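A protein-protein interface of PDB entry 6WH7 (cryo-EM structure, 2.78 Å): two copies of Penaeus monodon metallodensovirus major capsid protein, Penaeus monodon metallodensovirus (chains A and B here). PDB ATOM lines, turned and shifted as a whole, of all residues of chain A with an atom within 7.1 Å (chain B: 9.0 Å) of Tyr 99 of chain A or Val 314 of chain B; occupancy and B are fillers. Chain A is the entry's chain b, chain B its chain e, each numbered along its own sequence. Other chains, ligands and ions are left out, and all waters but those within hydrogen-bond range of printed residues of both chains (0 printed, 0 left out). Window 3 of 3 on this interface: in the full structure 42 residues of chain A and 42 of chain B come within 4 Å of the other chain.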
ATOM      1  N   ASN A  68      24.344  23.488   1.965  1.00  0.00           N
ATOM      2  CA  ASN A  68      23.522  22.955   0.901  1.00  0.00           C
ATOM      3  C   ASN A  68      23.317  24.038  -0.144  1.00  0.00           C
ATOM      4  O   ASN A  68      23.252  25.222   0.185  1.00  0.00           O
ATOM      5  CB  ASN A  68      22.190  22.489   1.490  1.00  0.00           C
ATOM      6  CG  ASN A  68      21.323  21.822   0.496  1.00  0.00           C
ATOM      7  OD1 ASN A  68      21.806  21.178  -0.425  1.00  0.00           O
ATOM      8  ND2 ASN A  68      20.024  21.992   0.647  1.00  0.00           N
ATOM      9  N   TYR A  94      20.592  15.581   6.883  1.00  0.00           N
ATOM     10  CA  TYR A  94      20.928  16.202   5.610  1.00  0.00           C
ATOM     11  C   TYR A  94      20.109  15.507   4.536  1.00  0.00           C
ATOM     12  O   TYR A  94      20.492  14.452   4.036  1.00  0.00           O
ATOM     13  CB  TYR A  94      22.426  16.067   5.364  1.00  0.00           C
ATOM     14  CG  TYR A  94      22.981  16.811   4.180  1.00  0.00           C
ATOM     15  CD1 TYR A  94      23.171  18.178   4.235  1.00  0.00           C
ATOM     16  CD2 TYR A  94      23.374  16.144   3.034  1.00  0.00           C
ATOM     17  CE1 TYR A  94      23.694  18.864   3.181  1.00  0.00           C
ATOM     18  CE2 TYR A  94      23.902  16.828   1.969  1.00  0.00           C
ATOM     19  CZ  TYR A  94      24.060  18.189   2.051  1.00  0.00           C
ATOM     20  OH  TYR A  94      24.586  18.889   0.998  1.00  0.00           O
ATOM     21  N   ASN A  95      19.027  16.144   4.120  1.00  0.00           N
ATOM     22  CA  ASN A  95      18.120  15.572   3.135  1.00  0.00           C
ATOM     23  C   ASN A  95      18.267  16.412   1.880  1.00  0.00           C
ATOM     24  O   ASN A  95      17.676  17.486   1.768  1.00  0.00           O
ATOM     25  CB  ASN A  95      16.686  15.583   3.645  1.00  0.00           C
ATOM     26  CG  ASN A  95      16.476  14.665   4.821  1.00  0.00           C
ATOM     27  OD1 ASN A  95      15.994  15.083   5.866  1.00  0.00           O
ATOM     28  ND2 ASN A  95      16.794  13.396   4.642  1.00  0.00           N
ATOM     29  N   THR A  96      19.021  15.894   0.925  1.00  0.00           N
ATOM     30  CA  THR A  96      19.331  16.625  -0.287  1.00  0.00           C
ATOM     31  C   THR A  96      19.615  15.609  -1.371  1.00  0.00           C
ATOM     32  O   THR A  96      20.229  14.578  -1.099  1.00  0.00           O
ATOM     33  CB  THR A  96      20.538  17.546  -0.090  1.00  0.00           C
ATOM     34  OG1 THR A  96      20.290  18.441   0.994  1.00  0.00           O
ATOM     35  CG2 THR A  96      20.789  18.356  -1.339  1.00  0.00           C
ATOM     36  N   GLY A  97      19.178  15.906  -2.589  1.00  0.00           N
ATOM     37  CA  GLY A  97      19.592  15.100  -3.722  1.00  0.00           C
ATOM     38  C   GLY A  97      19.352  13.629  -3.488  1.00  0.00           C
ATOM     39  O   GLY A  97      18.245  13.199  -3.152  1.00  0.00           O
ATOM     40  N   THR A  98      20.412  12.843  -3.654  1.00  0.00           N
ATOM     41  CA  THR A  98      20.330  11.404  -3.471  1.00  0.00           C
ATOM     42  C   THR A  98      20.439  10.996  -2.006  1.00  0.00           C
ATOM     43  O   THR A  98      19.986   9.905  -1.646  1.00  0.00           O
ATOM     44  CB  THR A  98      21.424  10.725  -4.297  1.00  0.00           C
ATOM     45  OG1 THR A  98      21.327  11.163  -5.655  1.00  0.00           O
ATOM     46  CG2 THR A  98      21.263   9.213  -4.285  1.00  0.00           C
ATOM     47  N   TYR A  99      20.998  11.859  -1.155  1.00  0.00           N
ATOM     48  CA  TYR A  99      21.241  11.510   0.242  1.00  0.00           C
ATOM     49  C   TYR A  99      19.980  11.003   0.925  1.00  0.00           C
ATOM     50  O   TYR A  99      19.926   9.860   1.387  1.00  0.00           O
ATOM     51  CB  TYR A  99      21.786  12.717   0.996  1.00  0.00           C
ATOM     52  CG  TYR A  99      23.110  13.208   0.496  1.00  0.00           C
ATOM     53  CD1 TYR A  99      24.296  12.698   0.991  1.00  0.00           C
ATOM     54  CD2 TYR A  99      23.172  14.194  -0.469  1.00  0.00           C
ATOM     55  CE1 TYR A  99      25.503  13.160   0.534  1.00  0.00           C
ATOM     56  CE2 TYR A  99      24.367  14.655  -0.930  1.00  0.00           C
ATOM     57  CZ  TYR A  99      25.530  14.137  -0.430  1.00  0.00           C
ATOM     58  OH  TYR A  99      26.719  14.617  -0.904  1.00  0.00           O
ATOM     59  N   GLY A 100      18.963  11.861   1.022  1.00  0.00           N
ATOM     60  CA  GLY A 100      17.735  11.479   1.697  1.00  0.00           C
ATOM     61  C   GLY A 100      17.135  10.191   1.177  1.00  0.00           C
ATOM     62  O   GLY A 100      16.520   9.437   1.932  1.00  0.00           O
ATOM     63  N   LEU A 101      17.303   9.917  -0.113  1.00  0.00           N
ATOM     64  CA  LEU A 101      16.803   8.672  -0.681  1.00  0.00           C
ATOM     65  C   LEU A 101      17.713   7.496  -0.362  1.00  0.00           C
ATOM     66  O   LEU A 101      17.248   6.353  -0.314  1.00  0.00           O
ATOM     67  CB  LEU A 101      16.651   8.798  -2.199  1.00  0.00           C
ATOM     68  CG  LEU A 101      15.627   9.722  -2.870  1.00  0.00           C
ATOM     69  CD1 LEU A 101      15.750  11.171  -2.446  1.00  0.00           C
ATOM     70  CD2 LEU A 101      15.786   9.624  -4.371  1.00  0.00           C
ATOM     71  N   SER A 102      18.998   7.756  -0.134  1.00  0.00           N
ATOM     72  CA  SER A 102      20.000   6.695  -0.139  1.00  0.00           C
ATOM     73  C   SER A 102      19.998   5.882   1.148  1.00  0.00           C
ATOM     74  O   SER A 102      20.034   4.648   1.106  1.00  0.00           O
ATOM     75  CB  SER A 102      21.386   7.294  -0.381  1.00  0.00           C
ATOM     76  OG  SER A 102      21.757   8.160   0.677  1.00  0.00           O
ATOM     77  N   GLY A 103      19.949   6.543   2.297  1.00  0.00           N
ATOM     78  CA  GLY A 103      20.350   5.878   3.526  1.00  0.00           C
ATOM     79  C   GLY A 103      20.398   6.841   4.690  1.00  0.00           C
ATOM     80  O   GLY A 103      19.667   7.837   4.720  1.00  0.00           O
ATOM     81  N   ASN A 104      21.260   6.527   5.654  1.00  0.00           N
ATOM     82  CA  ASN A 104      21.282   7.265   6.910  1.00  0.00           C
ATOM     83  C   ASN A 104      21.953   8.607   6.662  1.00  0.00           C
ATOM     84  O   ASN A 104      23.164   8.681   6.449  1.00  0.00           O
ATOM     85  CB  ASN A 104      22.031   6.460   7.969  1.00  0.00           C
ATOM     86  CG  ASN A 104      21.991   7.098   9.341  1.00  0.00           C
ATOM     87  OD1 ASN A 104      21.734   8.288   9.484  1.00  0.00           O
ATOM     88  ND2 ASN A 104      22.264   6.303  10.365  1.00  0.00           N
ATOM     89  N   VAL A 105      21.165   9.678   6.740  1.00  0.00           N
ATOM     90  CA  VAL A 105      21.642  11.028   6.496  1.00  0.00           C
ATOM     91  C   VAL A 105      21.896  11.795   7.773  1.00  0.00           C
ATOM     92  O   VAL A 105      22.202  12.988   7.718  1.00  0.00           O
ATOM     93  CB  VAL A 105      20.670  11.782   5.579  1.00  0.00           C
ATOM     94  CG1 VAL A 105      20.755  11.208   4.203  1.00  0.00           C
ATOM     95  CG2 VAL A 105      19.268  11.619   6.079  1.00  0.00           C
ATOM     96  N   HIS A 106      21.744  11.155   8.922  1.00  0.00           N
ATOM     97  CA  HIS A 106      21.971  11.825  10.189  1.00  0.00           C
ATOM     98  C   HIS A 106      23.439  12.173  10.351  1.00  0.00           C
ATOM     99  O   HIS A 106      24.322  11.431   9.922  1.00  0.00           O
ATOM    100  CB  HIS A 106      21.511  10.929  11.327  1.00  0.00           C
ATOM    101  CG  HIS A 106      20.058  10.591  11.265  1.00  0.00           C
ATOM    102  ND1 HIS A 106      19.075  11.459  11.684  1.00  0.00           N
ATOM    103  CD2 HIS A 106      19.417   9.505  10.774  1.00  0.00           C
ATOM    104  CE1 HIS A 106      17.892  10.903  11.492  1.00  0.00           C
ATOM    105  NE2 HIS A 106      18.072   9.721  10.935  1.00  0.00           N
ATOM    106  N   SER A 181      12.594  13.457   2.544  1.00  0.00           N
ATOM    107  CA  SER A 181      13.958  13.296   2.065  1.00  0.00           C
ATOM    108  C   SER A 181      14.412  14.458   1.207  1.00  0.00           C
ATOM    109  O   SER A 181      15.597  14.549   0.883  1.00  0.00           O
ATOM    110  CB  SER A 181      14.081  12.007   1.263  1.00  0.00           C
ATOM    111  OG  SER A 181      13.290  12.071   0.094  1.00  0.00           O
ATOM    112  N   GLU B 305      33.360  15.353  12.499  1.00  0.00           N
ATOM    113  CA  GLU B 305      33.506  16.465  11.575  1.00  0.00           C
ATOM    114  C   GLU B 305      32.170  17.138  11.307  1.00  0.00           C
ATOM    115  O   GLU B 305      31.139  16.480  11.166  1.00  0.00           O
ATOM    116  CB  GLU B 305      34.095  15.978  10.256  1.00  0.00           C
ATOM    117  CG  GLU B 305      35.488  15.439  10.362  1.00  0.00           C
ATOM    118  CD  GLU B 305      35.515  13.985  10.761  1.00  0.00           C
ATOM    119  OE1 GLU B 305      34.438  13.404  10.989  1.00  0.00           O
ATOM    120  OE2 GLU B 305      36.617  13.423  10.849  1.00  0.00           O
ATOM    121  N   GLY B 307      29.585  19.354   8.901  1.00  0.00           N
ATOM    122  CA  GLY B 307      29.275  19.354   7.498  1.00  0.00           C
ATOM    123  C   GLY B 307      28.841  17.997   7.007  1.00  0.00           C
ATOM    124  O   GLY B 307      28.573  17.067   7.768  1.00  0.00           O
ATOM    125  N   VAL B 308      28.770  17.892   5.681  1.00  0.00           N
ATOM    126  CA  VAL B 308      28.381  16.642   5.056  1.00  0.00           C
ATOM    127  C   VAL B 308      29.408  15.561   5.329  1.00  0.00           C
ATOM    128  O   VAL B 308      29.080  14.375   5.297  1.00  0.00           O
ATOM    129  CB  VAL B 308      28.168  16.869   3.551  1.00  0.00           C
ATOM    130  CG1 VAL B 308      27.730  15.597   2.863  1.00  0.00           C
ATOM    131  CG2 VAL B 308      27.161  17.958   3.342  1.00  0.00           C
ATOM    132  N   GLN B 309      30.644  15.944   5.636  1.00  0.00           N
ATOM    133  CA  GLN B 309      31.664  14.962   5.972  1.00  0.00           C
ATOM    134  C   GLN B 309      31.254  14.108   7.158  1.00  0.00           C
ATOM    135  O   GLN B 309      31.637  12.937   7.238  1.00  0.00           O
ATOM    136  CB  GLN B 309      32.976  15.670   6.272  1.00  0.00           C
ATOM    137  CG  GLN B 309      34.153  14.749   6.395  1.00  0.00           C
ATOM    138  CD  GLN B 309      35.425  15.504   6.613  1.00  0.00           C
ATOM    139  OE1 GLN B 309      35.421  16.724   6.707  1.00  0.00           O
ATOM    140  NE2 GLN B 309      36.532  14.794   6.644  1.00  0.00           N
ATOM    141  N   GLY B 310      30.474  14.664   8.079  1.00  0.00           N
ATOM    142  CA  GLY B 310      30.073  13.949   9.270  1.00  0.00           C
ATOM    143  C   GLY B 310      28.702  13.315   9.198  1.00  0.00           C
ATOM    144  O   GLY B 310      28.112  13.000  10.228  1.00  0.00           O
ATOM    145  N   ILE B 311      28.182  13.128   8.000  1.00  0.00           N
ATOM    146  CA  ILE B 311      26.920  12.424   7.815  1.00  0.00           C
ATOM    147  C   ILE B 311      27.178  10.926   7.841  1.00  0.00           C
ATOM    148  O   ILE B 311      28.153  10.448   7.259  1.00  0.00           O
ATOM    149  CB  ILE B 311      26.253  12.862   6.500  1.00  0.00           C
ATOM    150  CG1 ILE B 311      25.906  14.344   6.551  1.00  0.00           C
ATOM    151  CG2 ILE B 311      25.035  12.036   6.207  1.00  0.00           C
ATOM    152  CD1 ILE B 311      24.974  14.703   7.665  1.00  0.00           C
ATOM    153  N   ASN B 312      26.297  10.181   8.513  1.00  0.00           N
ATOM    154  CA  ASN B 312      26.516   8.752   8.731  1.00  0.00           C
ATOM    155  C   ASN B 312      26.836   8.010   7.441  1.00  0.00           C
ATOM    156  O   ASN B 312      27.797   7.236   7.382  1.00  0.00           O
ATOM    157  CB  ASN B 312      25.292   8.131   9.402  1.00  0.00           C
ATOM    158  CG  ASN B 312      25.206   8.449  10.874  1.00  0.00           C
ATOM    159  OD1 ASN B 312      26.210   8.705  11.520  1.00  0.00           O
ATOM    160  ND2 ASN B 312      23.997   8.426  11.416  1.00  0.00           N
ATOM    161  N   SER B 313      26.038   8.221   6.395  1.00  0.00           N
ATOM    162  CA  SER B 313      26.199   7.409   5.194  1.00  0.00           C
ATOM    163  C   SER B 313      27.485   7.749   4.458  1.00  0.00           C
ATOM    164  O   SER B 313      28.189   6.852   3.984  1.00  0.00           O
ATOM    165  CB  SER B 313      24.999   7.584   4.266  1.00  0.00           C
ATOM    166  OG  SER B 313      24.898   8.916   3.807  1.00  0.00           O
ATOM    167  N   VAL B 314      27.807   9.037   4.340  1.00  0.00           N
ATOM    168  CA  VAL B 314      28.978   9.445   3.574  1.00  0.00           C
ATOM    169  C   VAL B 314      30.235   9.592   4.418  1.00  0.00           C
ATOM    170  O   VAL B 314      31.322   9.782   3.854  1.00  0.00           O
ATOM    171  CB  VAL B 314      28.718  10.772   2.838  1.00  0.00           C
ATOM    172  CG1 VAL B 314      27.585  10.609   1.849  1.00  0.00           C
ATOM    173  CG2 VAL B 314      28.401  11.841   3.822  1.00  0.00           C
ATOM    174  N   HIS B 315      30.131   9.515   5.746  1.00  0.00           N
ATOM    175  CA  HIS B 315      31.331   9.604   6.570  1.00  0.00           C
ATOM    176  C   HIS B 315      32.213   8.382   6.403  1.00  0.00           C
ATOM    177  O   HIS B 315      33.435   8.479   6.546  1.00  0.00           O
ATOM    178  CB  HIS B 315      30.966   9.787   8.040  1.00  0.00           C
ATOM    179  CG  HIS B 315      32.146   9.988   8.936  1.00  0.00           C
ATOM    180  ND1 HIS B 315      32.871   8.939   9.457  1.00  0.00           N
ATOM    181  CD2 HIS B 315      32.735  11.115   9.395  1.00  0.00           C
ATOM    182  CE1 HIS B 315      33.852   9.412  10.202  1.00  0.00           C
ATOM    183  NE2 HIS B 315      33.791  10.732  10.182  1.00  0.00           N
ATOM    184  N   THR B 316      31.620   7.225   6.114  1.00  0.00           N
ATOM    185  CA  THR B 316      32.425   6.048   5.810  1.00  0.00           C
ATOM    186  C   THR B 316      33.369   6.326   4.651  1.00  0.00           C
ATOM    187  O   THR B 316      34.531   5.909   4.669  1.00  0.00           O
ATOM    188  CB  THR B 316      31.512   4.868   5.486  1.00  0.00           C
ATOM    189  OG1 THR B 316      30.694   5.199   4.359  1.00  0.00           O
ATOM    190  CG2 THR B 316      30.615   4.561   6.668  1.00  0.00           C
ATOM    191  N   ASN B 317      32.883   7.037   3.637  1.00  0.00           N
ATOM    192  CA  ASN B 317      33.692   7.376   2.475  1.00  0.00           C
ATOM    193  C   ASN B 317      34.576   8.586   2.741  1.00  0.00           C
ATOM    194  O   ASN B 317      35.745   8.606   2.346  1.00  0.00           O
ATOM    195  CB  ASN B 317      32.775   7.641   1.288  1.00  0.00           C
ATOM    196  CG  ASN B 317      31.973   6.422   0.898  1.00  0.00           C
ATOM    197  OD1 ASN B 317      32.383   5.292   1.147  1.00  0.00           O
ATOM    198  ND2 ASN B 317      30.808   6.646   0.306  1.00  0.00           N
ATOM    199  N   LEU B 318      34.033   9.598   3.407  1.00  0.00           N
ATOM    200  CA  LEU B 318      34.688  10.884   3.583  1.00  0.00           C
ATOM    201  C   LEU B 318      35.439  11.007   4.898  1.00  0.00           C
ATOM    202  O   LEU B 318      35.924  12.096   5.212  1.00  0.00           O
ATOM    203  CB  LEU B 318      33.667  12.009   3.467  1.00  0.00           C
ATOM    204  CG  LEU B 318      33.404  12.569   2.075  1.00  0.00           C
ATOM    205  CD1 LEU B 318      32.896  11.516   1.128  1.00  0.00           C
ATOM    206  CD2 LEU B 318      32.375  13.641   2.221  1.00  0.00           C
ATOM    207  N   ASN B 319      35.514   9.942   5.683  1.00  0.00           N
ATOM    208  CA  ASN B 319      36.367   9.955   6.859  1.00  0.00           C
ATOM    209  C   ASN B 319      37.781  10.357   6.454  1.00  0.00           C
ATOM    210  O   ASN B 319      38.313   9.816   5.476  1.00  0.00           O
ATOM    211  CB  ASN B 319      36.394   8.582   7.527  1.00  0.00           C
ATOM    212  CG  ASN B 319      37.052   8.615   8.885  1.00  0.00           C
ATOM    213  OD1 ASN B 319      36.934   9.591   9.618  1.00  0.00           O
ATOM    214  ND2 ASN B 319      37.772   7.557   9.219  1.00  0.00           N
ATOM    215  N   PRO B 320      38.407  11.299   7.153  1.00  0.00           N
ATOM    216  CA  PRO B 320      39.763  11.701   6.784  1.00  0.00           C
ATOM    217  C   PRO B 320      40.735  10.547   6.921  1.00  0.00           C
ATOM    218  O   PRO B 320      40.673   9.770   7.872  1.00  0.00           O
ATOM    219  CB  PRO B 320      40.078  12.813   7.783  1.00  0.00           C
ATOM    220  CG  PRO B 320      38.786  13.318   8.197  1.00  0.00           C
ATOM    221  CD  PRO B 320      37.860  12.160   8.208  1.00  0.00           C
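Tyr 99 of chain A touches one residue of chain B. Val 314 of chain B touches one residue of chain A. No residue of chain B comes within 4 Å of Gly 100 of chain A. No residue of chain B comes within 4 Å of Gly 103 of chain A. Printed residues of chain B within 4 Å of Asn 104 of chain A: Ile 311 (3.8 Å), Asn 312 (2.9 Å) and Ser 313 (2.9 Å). Printed residues of chain A within 4 Å of Val 308 of chain B: Tyr 94 (3.4 Å). Of the printed residues of chain B, Tyr 94 of chain A touches Val 308 and Ile 311. Thr 316 of chain B touches none of the printed residues of chain A. Gly 310 of chain B touches none of the printed residues of chain A. The nearest residue of chain B that does not touch Tyr 99 of chain A is Val 308 of chain B (4.02 Å). The nearest printed residue of chain A that does not touch Ser 313 of chain B is Ser 102 of chain A (4.5 Å).
The backbone carbonyl oxygen of His 106 of chain A lies within hydrogen-bond range of the backbone NH of Asn 312 of chain B (2.7 Å). ND2 of Asn 312 of chain B lies close to ND2 of Asn 104 of chain A (2.9 Å). The backbone carbonyl oxygen (O) of Asn 104 of chain A lies within hydrogen-bond range of the backbone NH (N) of Ser 313 of chain B (2.9 Å).
The backbone carbonyl oxygen (O) of Ser 313 of chain B is in hydrogen-bond range of the side-chain hydroxyl (OG1) of Thr 316 of chain B (3.0 Å). O of Tyr 99 of chain A lies within hydrogen-bond range of OG of Ser 102 of chain A (2.6 Å). N of His 106 of chain A sits close to OD1 of Asn 104 of chain A, at 2.9 Å. The backbone NH (N) of Tyr 94 of chain A sits at hydrogen-bond distance from the backbone carbonyl oxygen (O) of Val 105 of chain A (3.2 Å).
Of the 15 printed residues of chain B, 5 touch a printed residue of chain A. Printed residues of chain B that touch a printed residue of chain A: Val 308, Ile 311, Asn 312, Ser 313 and Val 314. Hydrophobic or aromatic side chains of chain A within 4 Å of the printed part of chain B: Tyr 94, Tyr 99 and His 106.
Val 308 of chain B touches Tyr 94 of chain A (CG2 to CZ, 3.4 Å). Ile 311 of chain B touches Tyr 94 of chain A (CD1 to CB, 3.7 Å). Val 314 of chain B touches Tyr 99 of chain A (CG1 to CE1, 3.5 Å). O of Asn 104 of chain A touches CG2 of Ile 311 of chain B, 3.8 Å away. Ile 311 of chain B touches Val 105 of chain A (CD1 to O, 3.3 Å). CA of Ile 311 of chain B touches O of His 106 of chain A (3.5 Å).
No position is printed for both chains. Of the 9 pairs that touch across the chains among the printed residues, none has its exchanged pair printed and touching as well.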
